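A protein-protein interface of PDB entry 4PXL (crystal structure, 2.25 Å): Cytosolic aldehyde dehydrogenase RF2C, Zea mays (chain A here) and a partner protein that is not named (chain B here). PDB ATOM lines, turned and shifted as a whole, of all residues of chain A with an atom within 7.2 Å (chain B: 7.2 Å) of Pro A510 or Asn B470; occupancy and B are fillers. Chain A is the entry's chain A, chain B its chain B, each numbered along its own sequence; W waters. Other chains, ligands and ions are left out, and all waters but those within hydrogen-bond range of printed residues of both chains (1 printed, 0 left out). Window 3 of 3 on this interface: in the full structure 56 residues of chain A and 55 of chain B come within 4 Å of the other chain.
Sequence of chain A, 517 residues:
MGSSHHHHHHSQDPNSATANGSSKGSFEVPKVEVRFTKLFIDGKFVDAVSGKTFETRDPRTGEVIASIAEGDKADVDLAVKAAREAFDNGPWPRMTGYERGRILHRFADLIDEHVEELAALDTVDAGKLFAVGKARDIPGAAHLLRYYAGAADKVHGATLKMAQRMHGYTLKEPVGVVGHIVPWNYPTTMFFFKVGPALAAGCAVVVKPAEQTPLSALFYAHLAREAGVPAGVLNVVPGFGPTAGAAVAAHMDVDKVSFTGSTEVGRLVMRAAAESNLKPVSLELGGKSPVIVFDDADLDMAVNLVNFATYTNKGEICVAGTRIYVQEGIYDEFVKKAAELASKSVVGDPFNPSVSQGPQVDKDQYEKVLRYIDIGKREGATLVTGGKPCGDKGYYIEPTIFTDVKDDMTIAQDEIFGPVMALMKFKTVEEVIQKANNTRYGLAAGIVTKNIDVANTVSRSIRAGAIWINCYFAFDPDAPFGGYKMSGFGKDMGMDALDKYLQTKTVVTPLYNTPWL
O of Thr A509 is in hydrogen-bond range of N of His A167. The backbone carbonyl oxygen of Trp B468 sits at hydrogen-bond distance from the backbone NH of Ile B447, at 2.9 Å. The backbone NH of Asn B470 lies within hydrogen-bond range of the backbone carbonyl oxygen of Ile B447. The backbone carbonyl oxygen of Thr B449 is in hydrogen-bond range of the side-chain amide nitrogen of Asn B470, 2.7 Å away. The backbone carbonyl oxygen (O) of Ile B469 sits at hydrogen-bond distance from the side-chain sulfur (SG) of Cys B471.
The backbone carbonyl oxygen (O) of Val A508 is in hydrogen-bond range of the backbone NH (N) of Ile B469 (2.8 Å). The backbone carbonyl oxygen of Val A508 lies within hydrogen-bond range of the side-chain sulfur of Cys B471, at 3.5 Å. OG1 of Thr A509 sits at hydrogen-bond distance from O of Ile B469.
Water W1 bridges the side-chain hydroxyl (OG1) of Thr A509 (2.8 Å) and the side-chain amide nitrogen (ND2) of Asn B470 (2.9 Å).
Among the printed residues, merely in contact across the chains: Pro A510 with Ile B469, Pro A510 with Asn B470, Val A508 with Ala B474, Val A508 with Trp B468 and Met A166 with Ala B474.
Printed residues of chain B within 4 Å of Val A508: Trp B468, Ile B469, Cys B471 and Ala B474. Printed residues of chain B within 4 Å of Thr A509: Ile B469. Pro A510 touches just these residues of chain B: Ile B469 (3.3 Å) and Asn B470 (3.4 Å). Ala B297 touches none of the printed residues of chain A. Printed residues of chain A within 4 Å of Ile B469: Val A508 (2.8 Å), Thr A509 (2.9 Å) and Pro A510 (3.3 Å). Of chain A, only Pro A510 comes within 4 Å of Asn B470. Of the printed residues of chain A, Cys B471 touches Val A508. Tyr B472 touches none of the printed residues of chain A. The nearest residue of chain B that does not touch Pro A510 is Cys B471 (4.1 Å).
Of the 8 printed residues of chain A, 4 touch a printed residue of chain B. Of the 17 printed residues of chain B, 5 touch a printed residue of chain A. Among the printed residues, 8 pairs touch across the chains. Among the printed residues, no Asp or Glu carboxylate lies within 4 Å of a Lys or Arg side-chain nitrogen of the other chain.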
ATOM      1  N   ARG A 165      25.654  30.162  27.894  1.00  0.00           N
ATOM      2  CA  ARG A 165      24.530  29.250  27.627  1.00  0.00           C
ATOM      3  C   ARG A 165      24.647  28.818  26.163  1.00  0.00           C
ATOM      4  O   ARG A 165      23.905  29.272  25.297  1.00  0.00           O
ATOM      5  CB  ARG A 165      23.189  29.933  27.969  1.00  0.00           C
ATOM      6  CG  ARG A 165      22.207  29.002  28.661  1.00  0.00           C
ATOM      7  CD  ARG A 165      20.974  29.714  29.191  1.00  0.00           C
ATOM      8  NE  ARG A 165      21.284  30.649  30.272  1.00  0.00           N
ATOM      9  CZ  ARG A 165      20.368  31.266  31.016  1.00  0.00           C
ATOM     10  NH1 ARG A 165      19.074  31.038  30.815  1.00  0.00           N
ATOM     11  NH2 ARG A 165      20.737  32.106  31.975  1.00  0.00           N
ATOM     12  N   MET A 166      25.670  27.993  25.899  1.00  0.00           N
ATOM     13  CA  MET A 166      26.077  27.534  24.570  1.00  0.00           C
ATOM     14  C   MET A 166      26.528  26.118  24.595  1.00  0.00           C
ATOM     15  O   MET A 166      27.049  25.653  25.599  1.00  0.00           O
ATOM     16  CB  MET A 166      27.273  28.368  24.075  1.00  0.00           C
ATOM     17  CG  MET A 166      26.878  29.678  23.506  1.00  0.00           C
ATOM     18  SD  MET A 166      28.361  30.627  23.163  1.00  0.00           S
ATOM     19  CE  MET A 166      27.624  32.217  22.718  1.00  0.00           C
ATOM     20  N   HIS A 167      26.380  25.448  23.461  1.00  0.00           N
ATOM     21  CA  HIS A 167      26.848  24.091  23.275  1.00  0.00           C
ATOM     22  C   HIS A 167      28.002  24.161  22.284  1.00  0.00           C
ATOM     23  O   HIS A 167      27.827  24.621  21.149  1.00  0.00           O
ATOM     24  CB  HIS A 167      25.721  23.184  22.735  1.00  0.00           C
ATOM     25  CG  HIS A 167      26.182  21.813  22.336  1.00  0.00           C
ATOM     26  ND1 HIS A 167      27.067  21.077  23.135  1.00  0.00           N
ATOM     27  CD2 HIS A 167      25.891  21.094  21.226  1.00  0.00           C
ATOM     28  CE1 HIS A 167      27.290  19.953  22.475  1.00  0.00           C
ATOM     29  NE2 HIS A 167      26.595  19.914  21.324  1.00  0.00           N
ATOM     30  N   VAL A 508      29.955  25.851  17.497  1.00  0.00           N
ATOM     31  CA  VAL A 508      29.240  26.407  18.678  1.00  0.00           C
ATOM     32  C   VAL A 508      27.874  26.920  18.286  1.00  0.00           C
ATOM     33  O   VAL A 508      27.734  27.570  17.254  1.00  0.00           O
ATOM     34  CB  VAL A 508      30.061  27.538  19.407  1.00  0.00           C
ATOM     35  CG1 VAL A 508      29.345  28.024  20.672  1.00  0.00           C
ATOM     36  CG2 VAL A 508      31.495  27.102  19.732  1.00  0.00           C
ATOM     37  N   THR A 509      26.879  26.688  19.154  1.00  0.00           N
ATOM     38  CA  THR A 509      25.499  27.160  18.979  1.00  0.00           C
ATOM     39  C   THR A 509      24.936  27.567  20.333  1.00  0.00           C
ATOM     40  O   THR A 509      25.331  26.971  21.331  1.00  0.00           O
ATOM     41  CB  THR A 509      24.638  26.110  18.210  1.00  0.00           C
ATOM     42  OG1 THR A 509      23.495  26.763  17.645  1.00  0.00           O
ATOM     43  CG2 THR A 509      24.206  24.901  19.068  1.00  0.00           C
ATOM     44  N   PRO A 510      24.028  28.563  20.435  1.00  0.00           N
ATOM     45  CA  PRO A 510      23.449  28.860  21.761  1.00  0.00           C
ATOM     46  C   PRO A 510      22.515  27.739  22.216  1.00  0.00           C
ATOM     47  O   PRO A 510      22.101  26.923  21.419  1.00  0.00           O
ATOM     48  CB  PRO A 510      22.663  30.157  21.553  1.00  0.00           C
ATOM     49  CG  PRO A 510      22.755  30.482  20.130  1.00  0.00           C
ATOM     50  CD  PRO A 510      23.435  29.401  19.380  1.00  0.00           C
ATOM     51  N   LEU A 511      22.163  27.734  23.481  1.00  0.00           N
ATOM     52  CA  LEU A 511      21.246  26.762  24.064  1.00  0.00           C
ATOM     53  C   LEU A 511      20.111  27.521  24.666  1.00  0.00           C
ATOM     54  O   LEU A 511      20.310  28.652  25.123  1.00  0.00           O
ATOM     55  CB  LEU A 511      21.933  25.970  25.170  1.00  0.00           C
ATOM     56  CG  LEU A 511      22.887  24.910  24.746  1.00  0.00           C
ATOM     57  CD1 LEU A 511      23.634  24.367  25.967  1.00  0.00           C
ATOM     58  CD2 LEU A 511      22.185  23.813  23.938  1.00  0.00           C
ATOM     59  N   TYR A 512      18.934  26.895  24.707  1.00  0.00           N
ATOM     60  CA  TYR A 512      17.723  27.498  25.261  1.00  0.00           C
ATOM     61  C   TYR A 512      17.081  26.544  26.270  1.00  0.00           C
ATOM     62  O   TYR A 512      16.903  25.357  25.980  1.00  0.00           O
ATOM     63  CB  TYR A 512      16.730  27.836  24.117  1.00  0.00           C
ATOM     64  CG  TYR A 512      17.329  28.771  23.080  1.00  0.00           C
ATOM     65  CD1 TYR A 512      17.389  30.142  23.302  1.00  0.00           C
ATOM     66  CD2 TYR A 512      17.892  28.274  21.908  1.00  0.00           C
ATOM     67  CE1 TYR A 512      17.995  30.998  22.387  1.00  0.00           C
ATOM     68  CE2 TYR A 512      18.526  29.118  20.997  1.00  0.00           C
ATOM     69  CZ  TYR A 512      18.551  30.484  21.227  1.00  0.00           C
ATOM     70  OH  TYR A 512      19.128  31.338  20.313  1.00  0.00           O
ATOM     71  N   ILE B 292      26.699  32.877   6.536  1.00  0.00           N
ATOM     72  CA  ILE B 292      25.677  32.373   5.628  1.00  0.00           C
ATOM     73  C   ILE B 292      24.315  32.428   6.281  1.00  0.00           C
ATOM     74  O   ILE B 292      24.112  31.798   7.316  1.00  0.00           O
ATOM     75  CB  ILE B 292      26.010  30.941   5.158  1.00  0.00           C
ATOM     76  CG1 ILE B 292      27.476  30.807   4.725  1.00  0.00           C
ATOM     77  CG2 ILE B 292      25.006  30.513   4.054  1.00  0.00           C
ATOM     78  CD1 ILE B 292      27.891  29.432   4.371  1.00  0.00           C
ATOM     79  N   ALA B 297      15.858  31.776   8.421  1.00  0.00           N
ATOM     80  CA  ALA B 297      16.324  32.629   9.518  1.00  0.00           C
ATOM     81  C   ALA B 297      15.308  33.682   9.926  1.00  0.00           C
ATOM     82  O   ALA B 297      14.553  34.173   9.079  1.00  0.00           O
ATOM     83  CB  ALA B 297      17.620  33.321   9.121  1.00  0.00           C
ATOM     84  N   MET B 301      16.895  38.946  13.779  1.00  0.00           N
ATOM     85  CA  MET B 301      17.981  38.279  14.510  1.00  0.00           C
ATOM     86  C   MET B 301      19.243  38.226  13.603  1.00  0.00           C
ATOM     87  O   MET B 301      20.301  38.679  14.030  1.00  0.00           O
ATOM     88  CB  MET B 301      17.528  36.875  14.986  1.00  0.00           C
ATOM     89  CG  MET B 301      18.649  35.985  15.509  1.00  0.00           C
ATOM     90  SD  MET B 301      19.527  35.088  14.194  1.00  0.00           S
ATOM     91  CE  MET B 301      20.060  33.660  15.076  1.00  0.00           C
ATOM     92  N   LEU B 305      22.700  40.008  13.947  1.00  0.00           N
ATOM     93  CA  LEU B 305      23.866  39.163  14.117  1.00  0.00           C
ATOM     94  C   LEU B 305      24.981  39.550  13.120  1.00  0.00           C
ATOM     95  O   LEU B 305      26.154  39.640  13.503  1.00  0.00           O
ATOM     96  CB  LEU B 305      23.481  37.680  13.982  1.00  0.00           C
ATOM     97  CG  LEU B 305      24.551  36.682  14.413  1.00  0.00           C
ATOM     98  CD1 LEU B 305      24.760  36.741  15.922  1.00  0.00           C
ATOM     99  CD2 LEU B 305      24.157  35.265  14.014  1.00  0.00           C
ATOM    100  N   GLY B 446      30.178  31.863  10.022  1.00  0.00           N
ATOM    101  CA  GLY B 446      28.898  31.932  10.698  1.00  0.00           C
ATOM    102  C   GLY B 446      27.819  31.321   9.830  1.00  0.00           C
ATOM    103  O   GLY B 446      27.865  31.450   8.610  1.00  0.00           O
ATOM    104  N   ILE B 447      26.875  30.600  10.447  1.00  0.00           N
ATOM    105  CA  ILE B 447      25.737  29.982   9.758  1.00  0.00           C
ATOM    106  C   ILE B 447      24.491  30.402  10.517  1.00  0.00           C
ATOM    107  O   ILE B 447      24.472  30.294  11.747  1.00  0.00           O
ATOM    108  CB  ILE B 447      25.831  28.438   9.700  1.00  0.00           C
ATOM    109  CG1 ILE B 447      27.140  27.971   9.057  1.00  0.00           C
ATOM    110  CG2 ILE B 447      24.607  27.839   8.993  1.00  0.00           C
ATOM    111  CD1 ILE B 447      27.427  26.499   9.405  1.00  0.00           C
ATOM    112  N   VAL B 448      23.473  30.887   9.794  1.00  0.00           N
ATOM    113  CA  VAL B 448      22.209  31.279  10.388  1.00  0.00           C
ATOM    114  C   VAL B 448      21.116  30.439   9.731  1.00  0.00           C
ATOM    115  O   VAL B 448      20.778  30.670   8.575  1.00  0.00           O
ATOM    116  CB  VAL B 448      21.891  32.810  10.340  1.00  0.00           C
ATOM    117  CG1 VAL B 448      20.695  33.130  11.233  1.00  0.00           C
ATOM    118  CG2 VAL B 448      23.102  33.641  10.766  1.00  0.00           C
ATOM    119  N   THR B 449      20.603  29.434  10.472  1.00  0.00           N
ATOM    120  CA  THR B 449      19.519  28.536  10.051  1.00  0.00           C
ATOM    121  C   THR B 449      18.878  27.896  11.297  1.00  0.00           C
ATOM    122  O   THR B 449      19.536  27.760  12.339  1.00  0.00           O
ATOM    123  CB  THR B 449      20.036  27.454   9.049  1.00  0.00           C
ATOM    124  OG1 THR B 449      18.917  26.811   8.460  1.00  0.00           O
ATOM    125  CG2 THR B 449      20.907  26.388   9.698  1.00  0.00           C
ATOM    126  N   LYS B 450      17.642  27.448  11.160  1.00  0.00           N
ATOM    127  CA  LYS B 450      16.944  26.740  12.231  1.00  0.00           C
ATOM    128  C   LYS B 450      16.983  25.242  11.981  1.00  0.00           C
ATOM    129  O   LYS B 450      16.745  24.474  12.902  1.00  0.00           O
ATOM    130  CB  LYS B 450      15.481  27.211  12.306  1.00  0.00           C
ATOM    131  CG  LYS B 450      15.302  28.687  12.677  1.00  0.00           C
ATOM    132  CD  LYS B 450      13.820  29.050  12.772  1.00  0.00           C
ATOM    133  CE  LYS B 450      13.625  30.519  13.025  1.00  0.00           C
ATOM    134  NZ  LYS B 450      12.237  30.949  12.690  1.00  0.00           N
ATOM    135  N   ASN B 451      17.238  24.828  10.727  1.00  0.00           N
ATOM    136  CA  ASN B 451      17.224  23.431  10.330  1.00  0.00           C
ATOM    137  C   ASN B 451      18.493  22.673  10.753  1.00  0.00           C
ATOM    138  O   ASN B 451      19.582  23.029  10.326  1.00  0.00           O
ATOM    139  CB  ASN B 451      16.959  23.309   8.829  1.00  0.00           C
ATOM    140  CG  ASN B 451      16.740  21.875   8.382  1.00  0.00           C
ATOM    141  OD1 ASN B 451      15.628  21.341   8.404  1.00  0.00           O
ATOM    142  ND2 ASN B 451      17.803  21.196   8.021  1.00  0.00           N
ATOM    143  N   ALA B 455      22.408  22.883   9.041  1.00  0.00           N
ATOM    144  CA  ALA B 455      23.465  23.287   9.979  1.00  0.00           C
ATOM    145  C   ALA B 455      24.594  22.251  10.023  1.00  0.00           C
ATOM    146  O   ALA B 455      25.759  22.627   9.890  1.00  0.00           O
ATOM    147  CB  ALA B 455      22.882  23.508  11.371  1.00  0.00           C
ATOM    148  N   TRP B 468      30.287  29.107  13.810  1.00  0.00           N
ATOM    149  CA  TRP B 468      29.351  29.701  14.766  1.00  0.00           C
ATOM    150  C   TRP B 468      27.955  29.634  14.199  1.00  0.00           C
ATOM    151  O   TRP B 468      27.669  30.265  13.182  1.00  0.00           O
ATOM    152  CB  TRP B 468      29.794  31.130  15.153  1.00  0.00           C
ATOM    153  CG  TRP B 468      31.114  31.154  15.858  1.00  0.00           C
ATOM    154  CD1 TRP B 468      31.572  30.239  16.770  1.00  0.00           C
ATOM    155  CD2 TRP B 468      32.184  32.092  15.659  1.00  0.00           C
ATOM    156  NE1 TRP B 468      32.859  30.550  17.154  1.00  0.00           N
ATOM    157  CE2 TRP B 468      33.260  31.684  16.490  1.00  0.00           C
ATOM    158  CE3 TRP B 468      32.359  33.212  14.832  1.00  0.00           C
ATOM    159  CZ2 TRP B 468      34.459  32.401  16.567  1.00  0.00           C
ATOM    160  CZ3 TRP B 468      33.556  33.904  14.893  1.00  0.00           C
ATOM    161  CH2 TRP B 468      34.588  33.500  15.755  1.00  0.00           C
ATOM    162  N   ILE B 469      27.118  28.782  14.809  1.00  0.00           N
ATOM    163  CA  ILE B 469      25.755  28.564  14.350  1.00  0.00           C
ATOM    164  C   ILE B 469      24.794  29.381  15.175  1.00  0.00           C
ATOM    165  O   ILE B 469      24.669  29.128  16.369  1.00  0.00           O
ATOM    166  CB  ILE B 469      25.396  27.050  14.317  1.00  0.00           C
ATOM    167  CG1 ILE B 469      26.471  26.259  13.488  1.00  0.00           C
ATOM    168  CG2 ILE B 469      23.959  26.853  13.739  1.00  0.00           C
ATOM    169  CD1 ILE B 469      26.355  24.734  13.531  1.00  0.00           C
ATOM    170  N   ASN B 470      24.110  30.361  14.540  1.00  0.00           N
ATOM    171  CA  ASN B 470      23.104  31.228  15.197  1.00  0.00           C
ATOM    172  C   ASN B 470      23.673  32.066  16.348  1.00  0.00           C
ATOM    173  O   ASN B 470      22.955  32.429  17.292  1.00  0.00           O
ATOM    174  CB  ASN B 470      21.870  30.396  15.655  1.00  0.00           C
ATOM    175  CG  ASN B 470      21.162  29.759  14.505  1.00  0.00           C
ATOM    176  OD1 ASN B 470      21.098  30.322  13.418  1.00  0.00           O
ATOM    177  ND2 ASN B 470      20.641  28.570  14.705  1.00  0.00           N
ATOM    178  N   CYS B 471      24.972  32.353  16.265  1.00  0.00           N
ATOM    179  CA  CYS B 471      25.739  33.166  17.208  1.00  0.00           C
ATOM    180  C   CYS B 471      26.972  33.630  16.446  1.00  0.00           C
ATOM    181  O   CYS B 471      27.193  33.198  15.310  1.00  0.00           O
ATOM    182  CB  CYS B 471      26.111  32.363  18.459  1.00  0.00           C
ATOM    183  SG  CYS B 471      27.151  30.902  18.134  1.00  0.00           S
ATOM    184  N   TYR B 472      27.767  34.491  17.061  1.00  0.00           N
ATOM    185  CA  TYR B 472      29.007  34.954  16.461  1.00  0.00           C
ATOM    186  C   TYR B 472      30.008  35.316  17.526  1.00  0.00           C
ATOM    187  O   TYR B 472      29.593  35.684  18.626  1.00  0.00           O
ATOM    188  CB  TYR B 472      28.792  36.117  15.460  1.00  0.00           C
ATOM    189  CG  TYR B 472      29.796  36.028  14.333  1.00  0.00           C
ATOM    190  CD1 TYR B 472      29.652  35.076  13.321  1.00  0.00           C
ATOM    191  CD2 TYR B 472      30.958  36.799  14.345  1.00  0.00           C
ATOM    192  CE1 TYR B 472      30.601  34.938  12.317  1.00  0.00           C
ATOM    193  CE2 TYR B 472      31.901  36.696  13.320  1.00  0.00           C
ATOM    194  CZ  TYR B 472      31.719  35.756  12.312  1.00  0.00           C
ATOM    195  OH  TYR B 472      32.634  35.619  11.300  1.00  0.00           O
ATOM    196  N   ALA B 474      31.774  33.365  19.261  1.00  0.00           N
ATOM    197  CA  ALA B 474      31.499  32.473  20.386  1.00  0.00           C
ATOM    198  C   ALA B 474      32.793  31.867  20.923  1.00  0.00           C
ATOM    199  O   ALA B 474      32.923  30.646  21.028  1.00  0.00           O
ATOM    200  CB  ALA B 474      30.512  31.391  19.967  1.00  0.00           C
HETATM  201  O   HOH W   1      20.824  27.689  17.456  1.00  0.00           O
